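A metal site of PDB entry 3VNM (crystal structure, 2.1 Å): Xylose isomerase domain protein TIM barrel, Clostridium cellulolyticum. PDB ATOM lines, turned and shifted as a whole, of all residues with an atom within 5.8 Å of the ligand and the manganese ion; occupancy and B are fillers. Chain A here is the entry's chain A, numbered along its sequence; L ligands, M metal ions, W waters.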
ATOM      1  N   TYR A   6      15.923   5.078 -11.178  1.00  0.00           N
ATOM      2  CA  TYR A   6      14.851   5.575 -12.051  1.00  0.00           C
ATOM      3  C   TYR A   6      13.759   4.462 -12.107  1.00  0.00           C
ATOM      4  O   TYR A   6      14.070   3.279 -12.317  1.00  0.00           O
ATOM      5  CB  TYR A   6      15.414   5.854 -13.439  1.00  0.00           C
ATOM      6  CG  TYR A   6      14.575   6.702 -14.397  1.00  0.00           C
ATOM      7  CD1 TYR A   6      13.639   7.638 -13.932  1.00  0.00           C
ATOM      8  CD2 TYR A   6      14.798   6.620 -15.768  1.00  0.00           C
ATOM      9  CE1 TYR A   6      12.933   8.470 -14.817  1.00  0.00           C
ATOM     10  CE2 TYR A   6      14.133   7.452 -16.668  1.00  0.00           C
ATOM     11  CZ  TYR A   6      13.190   8.367 -16.181  1.00  0.00           C
ATOM     12  OH  TYR A   6      12.531   9.156 -17.096  1.00  0.00           O
ATOM     13  N   TRP A  14       6.630   6.095 -20.125  1.00  0.00           N
ATOM     14  CA  TRP A  14       7.130   7.237 -19.350  1.00  0.00           C
ATOM     15  C   TRP A  14       6.146   7.774 -18.302  1.00  0.00           C
ATOM     16  O   TRP A  14       5.927   8.978 -18.206  1.00  0.00           O
ATOM     17  CB  TRP A  14       7.607   8.389 -20.280  1.00  0.00           C
ATOM     18  CG  TRP A  14       8.771   7.952 -21.197  1.00  0.00           C
ATOM     19  CD1 TRP A  14       8.761   7.914 -22.567  1.00  0.00           C
ATOM     20  CD2 TRP A  14      10.080   7.492 -20.795  1.00  0.00           C
ATOM     21  NE1 TRP A  14       9.979   7.457 -23.054  1.00  0.00           N
ATOM     22  CE2 TRP A  14      10.803   7.196 -21.988  1.00  0.00           C
ATOM     23  CE3 TRP A  14      10.696   7.286 -19.546  1.00  0.00           C
ATOM     24  CZ2 TRP A  14      12.126   6.717 -21.964  1.00  0.00           C
ATOM     25  CZ3 TRP A  14      12.024   6.801 -19.527  1.00  0.00           C
ATOM     26  CH2 TRP A  14      12.718   6.519 -20.733  1.00  0.00           C
ATOM     27  N   GLU A  34      13.680   8.311  -8.764  1.00  0.00           N
ATOM     28  CA  GLU A  34      13.617   9.354  -9.810  1.00  0.00           C
ATOM     29  C   GLU A  34      12.430   9.007 -10.680  1.00  0.00           C
ATOM     30  O   GLU A  34      12.276   7.854 -11.055  1.00  0.00           O
ATOM     31  CB  GLU A  34      14.916   9.403 -10.637  1.00  0.00           C
ATOM     32  CG  GLU A  34      14.858  10.418 -11.807  1.00  0.00           C
ATOM     33  CD  GLU A  34      16.257  11.027 -12.163  1.00  0.00           C
ATOM     34  OE1 GLU A  34      16.998  11.430 -11.243  1.00  0.00           O
ATOM     35  OE2 GLU A  34      16.579  11.093 -13.355  1.00  0.00           O
ATOM     36  N   GLY A  65      13.241  13.307 -14.106  1.00  0.00           N
ATOM     37  CA  GLY A  65      13.917  13.308 -15.382  1.00  0.00           C
ATOM     38  C   GLY A  65      12.902  13.636 -16.472  1.00  0.00           C
ATOM     39  O   GLY A  65      11.704  13.354 -16.331  1.00  0.00           O
ATOM     40  N   HIS A  66      13.364  14.222 -17.576  1.00  0.00           N
ATOM     41  CA  HIS A  66      12.448  14.496 -18.685  1.00  0.00           C
ATOM     42  C   HIS A  66      13.094  14.453 -20.057  1.00  0.00           C
ATOM     43  O   HIS A  66      14.165  15.018 -20.270  1.00  0.00           O
ATOM     44  CB  HIS A  66      11.774  15.868 -18.538  1.00  0.00           C
ATOM     45  CG  HIS A  66      10.604  16.047 -19.448  1.00  0.00           C
ATOM     46  ND1 HIS A  66      10.393  17.200 -20.176  1.00  0.00           N
ATOM     47  CD2 HIS A  66       9.564  15.232 -19.724  1.00  0.00           C
ATOM     48  CE1 HIS A  66       9.274  17.087 -20.858  1.00  0.00           C
ATOM     49  NE2 HIS A  66       8.752  15.896 -20.599  1.00  0.00           N
ATOM     50  N   GLY A  67      12.414  13.798 -20.985  1.00  0.00           N
ATOM     51  CA  GLY A  67      12.840  13.744 -22.368  1.00  0.00           C
ATOM     52  C   GLY A  67      11.845  14.689 -23.039  1.00  0.00           C
ATOM     53  O   GLY A  67      10.717  14.283 -23.289  1.00  0.00           O
ATOM     54  N   GLY A 105      16.156  16.907 -14.441  1.00  0.00           N
ATOM     55  CA  GLY A 105      17.296  16.721 -15.306  1.00  0.00           C
ATOM     56  C   GLY A 105      16.932  16.078 -16.598  1.00  0.00           C
ATOM     57  O   GLY A 105      15.794  15.581 -16.750  1.00  0.00           O
ATOM     58  N   GLY A 106      17.901  16.095 -17.511  1.00  0.00           N
ATOM     59  CA  GLY A 106      17.763  15.516 -18.841  1.00  0.00           C
ATOM     60  C   GLY A 106      18.144  16.496 -19.953  1.00  0.00           C
ATOM     61  O   GLY A 106      18.854  17.498 -19.720  1.00  0.00           O
ATOM     62  N   ALA A 107      17.652  16.259 -21.157  1.00  0.00           N
ATOM     63  CA  ALA A 107      17.967  17.110 -22.309  1.00  0.00           C
ATOM     64  C   ALA A 107      17.060  18.320 -22.266  1.00  0.00           C
ATOM     65  O   ALA A 107      16.393  18.616 -23.241  1.00  0.00           O
ATOM     66  CB  ALA A 107      17.721  16.341 -23.618  1.00  0.00           C
ATOM     67  N   TRP A 112      13.995  15.240 -26.901  1.00  0.00           N
ATOM     68  CA  TRP A 112      14.535  13.878 -26.983  1.00  0.00           C
ATOM     69  C   TRP A 112      13.397  12.863 -27.045  1.00  0.00           C
ATOM     70  O   TRP A 112      12.410  13.000 -26.353  1.00  0.00           O
ATOM     71  CB  TRP A 112      15.356  13.603 -25.712  1.00  0.00           C
ATOM     72  CG  TRP A 112      15.930  12.218 -25.575  1.00  0.00           C
ATOM     73  CD1 TRP A 112      17.183  11.798 -25.970  1.00  0.00           C
ATOM     74  CD2 TRP A 112      15.283  11.070 -25.018  1.00  0.00           C
ATOM     75  NE1 TRP A 112      17.344  10.453 -25.700  1.00  0.00           N
ATOM     76  CE2 TRP A 112      16.195   9.977 -25.117  1.00  0.00           C
ATOM     77  CE3 TRP A 112      14.019  10.851 -24.454  1.00  0.00           C
ATOM     78  CZ2 TRP A 112      15.881   8.690 -24.664  1.00  0.00           C
ATOM     79  CZ3 TRP A 112      13.703   9.546 -23.999  1.00  0.00           C
ATOM     80  CH2 TRP A 112      14.633   8.492 -24.112  1.00  0.00           C
ATOM     81  N   GLU A 150      21.716  17.500 -18.987  1.00  0.00           N
ATOM     82  CA  GLU A 150      22.433  16.237 -19.176  1.00  0.00           C
ATOM     83  C   GLU A 150      23.219  16.129 -20.481  1.00  0.00           C
ATOM     84  O   GLU A 150      22.675  16.333 -21.560  1.00  0.00           O
ATOM     85  CB  GLU A 150      21.457  15.029 -19.064  1.00  0.00           C
ATOM     86  CG  GLU A 150      22.115  13.675 -19.317  1.00  0.00           C
ATOM     87  CD  GLU A 150      21.112  12.471 -19.201  1.00  0.00           C
ATOM     88  OE1 GLU A 150      19.886  12.640 -19.320  1.00  0.00           O
ATOM     89  OE2 GLU A 150      21.558  11.345 -18.997  1.00  0.00           O
ATOM     90  N   LEU A 152      24.658  14.237 -23.430  1.00  0.00           N
ATOM     91  CA  LEU A 152      24.300  12.977 -24.079  1.00  0.00           C
ATOM     92  C   LEU A 152      25.189  12.572 -25.237  1.00  0.00           C
ATOM     93  O   LEU A 152      25.918  13.409 -25.842  1.00  0.00           O
ATOM     94  CB  LEU A 152      22.878  13.045 -24.599  1.00  0.00           C
ATOM     95  CG  LEU A 152      21.820  13.534 -23.611  1.00  0.00           C
ATOM     96  CD1 LEU A 152      20.596  13.857 -24.390  1.00  0.00           C
ATOM     97  CD2 LEU A 152      21.545  12.480 -22.543  1.00  0.00           C
ATOM     98  N   ASN A 153      25.104  11.288 -25.617  1.00  0.00           N
ATOM     99  CA  ASN A 153      25.919  10.860 -26.724  1.00  0.00           C
ATOM    100  C   ASN A 153      25.329  11.413 -28.041  1.00  0.00           C
ATOM    101  O   ASN A 153      24.152  11.828 -28.141  1.00  0.00           O
ATOM    102  CB  ASN A 153      26.056   9.326 -26.759  1.00  0.00           C
ATOM    103  CG  ASN A 153      24.752   8.614 -27.091  1.00  0.00           C
ATOM    104  OD1 ASN A 153      24.252   8.705 -28.208  1.00  0.00           O
ATOM    105  ND2 ASN A 153      24.194   7.889 -26.111  1.00  0.00           N
ATOM    106  N   GLU A 156      21.921  10.760 -29.594  1.00  0.00           N
ATOM    107  CA  GLU A 156      20.711  11.186 -28.905  1.00  0.00           C
ATOM    108  C   GLU A 156      20.569  12.694 -28.755  1.00  0.00           C
ATOM    109  O   GLU A 156      19.561  13.165 -28.231  1.00  0.00           O
ATOM    110  CB  GLU A 156      20.683  10.531 -27.490  1.00  0.00           C
ATOM    111  CG  GLU A 156      20.535   8.995 -27.538  1.00  0.00           C
ATOM    112  CD  GLU A 156      20.336   8.393 -26.147  1.00  0.00           C
ATOM    113  OE1 GLU A 156      19.400   8.830 -25.427  1.00  0.00           O
ATOM    114  OE2 GLU A 156      21.125   7.503 -25.755  1.00  0.00           O
ATOM    115  N   MET A 181      25.002  17.764 -15.881  1.00  0.00           N
ATOM    116  CA  MET A 181      24.626  16.460 -15.350  1.00  0.00           C
ATOM    117  C   MET A 181      25.373  15.475 -16.219  1.00  0.00           C
ATOM    118  O   MET A 181      25.347  15.603 -17.425  1.00  0.00           O
ATOM    119  CB  MET A 181      23.121  16.309 -15.502  1.00  0.00           C
ATOM    120  CG  MET A 181      22.537  14.902 -15.278  1.00  0.00           C
ATOM    121  SD  MET A 181      20.735  14.952 -15.374  1.00  0.00           S
ATOM    122  CE  MET A 181      20.381  13.103 -15.634  1.00  0.00           C
ATOM    123  N   ASP A 183      26.389  11.230 -17.160  1.00  0.00           N
ATOM    124  CA  ASP A 183      25.778   9.919 -17.169  1.00  0.00           C
ATOM    125  C   ASP A 183      26.845   8.924 -17.670  1.00  0.00           C
ATOM    126  O   ASP A 183      27.332   9.035 -18.778  1.00  0.00           O
ATOM    127  CB  ASP A 183      24.548   9.981 -18.087  1.00  0.00           C
ATOM    128  CG  ASP A 183      23.879   8.611 -18.352  1.00  0.00           C
ATOM    129  OD1 ASP A 183      24.545   7.563 -18.403  1.00  0.00           O
ATOM    130  OD2 ASP A 183      22.655   8.614 -18.587  1.00  0.00           O
ATOM    131  N   PHE A 185      26.767   6.038 -18.897  1.00  0.00           N
ATOM    132  CA  PHE A 185      26.487   5.437 -20.194  1.00  0.00           C
ATOM    133  C   PHE A 185      26.856   6.352 -21.416  1.00  0.00           C
ATOM    134  O   PHE A 185      27.292   5.854 -22.486  1.00  0.00           O
ATOM    135  CB  PHE A 185      24.984   5.057 -20.289  1.00  0.00           C
ATOM    136  CG  PHE A 185      24.509   4.709 -21.693  1.00  0.00           C
ATOM    137  CD1 PHE A 185      24.909   3.526 -22.325  1.00  0.00           C
ATOM    138  CD2 PHE A 185      23.718   5.589 -22.388  1.00  0.00           C
ATOM    139  CE1 PHE A 185      24.538   3.233 -23.622  1.00  0.00           C
ATOM    140  CE2 PHE A 185      23.329   5.332 -23.696  1.00  0.00           C
ATOM    141  CZ  PHE A 185      23.746   4.123 -24.334  1.00  0.00           C
ATOM    142  N   HIS A 186      26.656   7.670 -21.250  1.00  0.00           N
ATOM    143  CA  HIS A 186      26.937   8.622 -22.334  1.00  0.00           C
ATOM    144  C   HIS A 186      28.406   9.020 -22.367  1.00  0.00           C
ATOM    145  O   HIS A 186      28.953   9.273 -23.439  1.00  0.00           O
ATOM    146  CB  HIS A 186      26.066   9.887 -22.202  1.00  0.00           C
ATOM    147  CG  HIS A 186      24.604   9.636 -22.456  1.00  0.00           C
ATOM    148  ND1 HIS A 186      24.139   9.157 -23.660  1.00  0.00           N
ATOM    149  CD2 HIS A 186      23.539   9.717 -21.627  1.00  0.00           C
ATOM    150  CE1 HIS A 186      22.834   8.955 -23.567  1.00  0.00           C
ATOM    151  NE2 HIS A 186      22.445   9.283 -22.347  1.00  0.00           N
ATOM    152  N   HIS A 209      23.845  10.172 -13.368  1.00  0.00           N
ATOM    153  CA  HIS A 209      23.105   8.948 -13.737  1.00  0.00           C
ATOM    154  C   HIS A 209      24.137   7.840 -13.927  1.00  0.00           C
ATOM    155  O   HIS A 209      25.227   8.072 -14.503  1.00  0.00           O
ATOM    156  CB  HIS A 209      22.437   9.047 -15.082  1.00  0.00           C
ATOM    157  CG  HIS A 209      21.056   9.582 -15.066  1.00  0.00           C
ATOM    158  ND1 HIS A 209      20.339   9.794 -16.231  1.00  0.00           N
ATOM    159  CD2 HIS A 209      20.261  10.001 -14.050  1.00  0.00           C
ATOM    160  CE1 HIS A 209      19.174  10.331 -15.924  1.00  0.00           C
ATOM    161  NE2 HIS A 209      19.101  10.473 -14.612  1.00  0.00           N
ATOM    162  N   ARG A 215      23.791  -0.359 -20.445  1.00  0.00           N
ATOM    163  CA  ARG A 215      22.648   0.064 -19.609  1.00  0.00           C
ATOM    164  C   ARG A 215      22.166  -0.964 -18.589  1.00  0.00           C
ATOM    165  O   ARG A 215      21.012  -0.913 -18.138  1.00  0.00           O
ATOM    166  CB  ARG A 215      21.484   0.477 -20.491  1.00  0.00           C
ATOM    167  CG  ARG A 215      21.785   1.657 -21.459  1.00  0.00           C
ATOM    168  CD  ARG A 215      21.529   3.000 -20.740  1.00  0.00           C
ATOM    169  NE  ARG A 215      20.865   3.823 -21.670  1.00  0.00           N
ATOM    170  CZ  ARG A 215      20.513   5.072 -21.498  1.00  0.00           C
ATOM    171  NH1 ARG A 215      20.758   5.723 -20.356  1.00  0.00           N
ATOM    172  NH2 ARG A 215      19.969   5.698 -22.549  1.00  0.00           N
ATOM    173  N   GLU A 244      20.193   4.300 -13.702  1.00  0.00           N
ATOM    174  CA  GLU A 244      19.162   4.333 -14.702  1.00  0.00           C
ATOM    175  C   GLU A 244      19.262   3.077 -15.602  1.00  0.00           C
ATOM    176  O   GLU A 244      19.466   3.149 -16.815  1.00  0.00           O
ATOM    177  CB  GLU A 244      19.415   5.616 -15.472  1.00  0.00           C
ATOM    178  CG  GLU A 244      18.419   5.969 -16.430  1.00  0.00           C
ATOM    179  CD  GLU A 244      18.840   7.245 -17.183  1.00  0.00           C
ATOM    180  OE1 GLU A 244      20.022   7.335 -17.573  1.00  0.00           O
ATOM    181  OE2 GLU A 244      17.978   8.100 -17.378  1.00  0.00           O
ATOM    182  N   PHE A 246      18.192  -0.002 -17.986  1.00  0.00           N
ATOM    183  CA  PHE A 246      17.154  -0.287 -18.960  1.00  0.00           C
ATOM    184  C   PHE A 246      17.494  -1.655 -19.501  1.00  0.00           C
ATOM    185  O   PHE A 246      18.308  -1.777 -20.416  1.00  0.00           O
ATOM    186  CB  PHE A 246      17.164   0.727 -20.113  1.00  0.00           C
ATOM    187  CG  PHE A 246      16.725   2.126 -19.710  1.00  0.00           C
ATOM    188  CD1 PHE A 246      15.389   2.406 -19.442  1.00  0.00           C
ATOM    189  CD2 PHE A 246      17.668   3.141 -19.560  1.00  0.00           C
ATOM    190  CE1 PHE A 246      14.974   3.703 -19.034  1.00  0.00           C
ATOM    191  CE2 PHE A 246      17.279   4.447 -19.136  1.00  0.00           C
ATOM    192  CZ  PHE A 246      15.949   4.721 -18.874  1.00  0.00           C
ATOM    193  N   ILE A 257      14.855   3.978 -25.743  1.00  0.00           N
ATOM    194  CA  ILE A 257      16.164   3.582 -25.265  1.00  0.00           C
ATOM    195  C   ILE A 257      16.844   2.620 -26.244  1.00  0.00           C
ATOM    196  O   ILE A 257      18.026   2.361 -26.154  1.00  0.00           O
ATOM    197  CB  ILE A 257      16.027   2.923 -23.844  1.00  0.00           C
ATOM    198  CG1 ILE A 257      15.343   3.910 -22.861  1.00  0.00           C
ATOM    199  CG2 ILE A 257      17.374   2.541 -23.278  1.00  0.00           C
ATOM    200  CD1 ILE A 257      16.120   5.223 -22.641  1.00  0.00           C
HETATM  201  C1  LIG L   1      18.634   8.844 -22.065  1.00  0.00           C
HETATM  202  O1  LIG L   1      19.719   8.508 -22.925  1.00  0.00           O
HETATM  203  C2  LIG L   1      19.113   9.566 -20.794  1.00  0.00           C
HETATM  204  O2  LIG L   1      20.076   9.176 -20.139  1.00  0.00           O
HETATM  205  C3  LIG L   1      18.026  10.379 -20.097  1.00  0.00           C
HETATM  206  O3  LIG L   1      18.442  10.549 -18.738  1.00  0.00           O
HETATM  207  C4  LIG L   1      16.737   9.564 -20.139  1.00  0.00           C
HETATM  208  O4  LIG L   1      17.023   8.222 -19.725  1.00  0.00           O
HETATM  209  C5  LIG L   1      15.677  10.215 -19.238  1.00  0.00           C
HETATM  210  O5  LIG L   1      14.574   9.325 -19.060  1.00  0.00           O
HETATM  211  C6  LIG L   1      15.170  11.502 -19.892  1.00  0.00           C
HETATM  212  O6  LIG L   1      16.235  12.440 -20.038  1.00  0.00           O
HETATM  213 MN    MN M   1      20.678   9.470 -18.235  1.00  0.00          MN
HETATM  214  O   HOH W   1      16.735  12.760 -17.470  1.00  0.00           O
HETATM  215  O   HOH W   2      15.856  10.171 -15.889  1.00  0.00           O
HETATM  216  O   HOH W   3      12.074  10.255 -21.194  1.00  0.00           O
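Trp 14 touches the ligand.
Gly 67 touches the ligand (N to C6, 3.7 Å).
Gly 106 touches the ligand (CA to O6, 3.6 Å).
Trp 112 touches the ligand.
Phe 246 touches the ligand (CZ to O4, 3.8 Å).
Hydrophobic or aromatic side chains within 4 Å of the ligand: Tyr 6, Trp 14, Trp 112, His 186, His 209 and Phe 246.
Of the 23 residues printed, 14 come within 4 Å of the ligand.
The nearest printed residue that does not touch the ligand is Leu 152 (4.2 Å).
Four residues have an atom within 4 Å of the manganese ion: Glu 150, Asp 183, His 209 and Glu 244.
The side-chain carboxylate of Glu 156 lies within hydrogen-bond range of an oxygen (O1) of the ligand (2.5 Å).
OH of Tyr 6 sits at hydrogen-bond distance from O5 of the ligand, at 2.8 Å.
NH2 of Arg 215 is in hydrogen-bond range of O1 of the ligand, 2.8 Å away.
NE2 of His 186 is in hydrogen-bond range of O1 of the ligand, 2.9 Å away.
An oxygen (O6) of the ligand lies within hydrogen-bond range of the backbone carbonyl oxygen (O) of His 66 (3.3 Å).
NE2 of His 209 sits at hydrogen-bond distance from OE2 of Glu 34 (2.9 Å).
The side-chain carboxylate (OD2) of Asp 183 lies close to the guanidinium group (NH1) of Arg 215, at 3.9 Å.
The side-chain carboxylate (OD1) of Asp 183 sits at hydrogen-bond distance from the backbone NH (N) of Phe 185, at 2.7 Å.
The guanidinium group (NH1) of Arg 215 lies close to the side-chain carboxylate (OE1) of Glu 244 (3.3 Å).
OE2 of Glu 156 lies within salt-bridge range of NH2 of Arg 215 (3.9 Å).
The side-chain amide nitrogen (ND2) of Asn 153 is in hydrogen-bond range of the side-chain carboxylate (OE2) of Glu 156 (3.1 Å).
The side-chain amide nitrogen of Asn 153 lies within hydrogen-bond range of a ring nitrogen (ND1) of His 186.
O of Gly 105 sits at hydrogen-bond distance from N of His 66 (2.9 Å).
The manganese ion is bound by O2 of the ligand (2.0 Å), ND1 of His 209 (2.1 Å), OD2 of Asp 183 (2.2 Å), OE2 of Glu 150 (2.2 Å), OE1 of Glu 244 (2.3 Å) and O3 of the ligand (2.5 Å).
Water W1 lies within hydrogen-bond range of an oxygen (O6) of the ligand (2.6 Å) and the backbone carbonyl oxygen of Gly 105 (3.1 Å).
Water W2 lies within hydrogen-bond range of the side-chain carboxylate of Glu 34 (2.8 Å), the side-chain carboxylate of Glu 244 (3.3 Å) and a ring nitrogen (NE2) of His 209 (3.5 Å).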
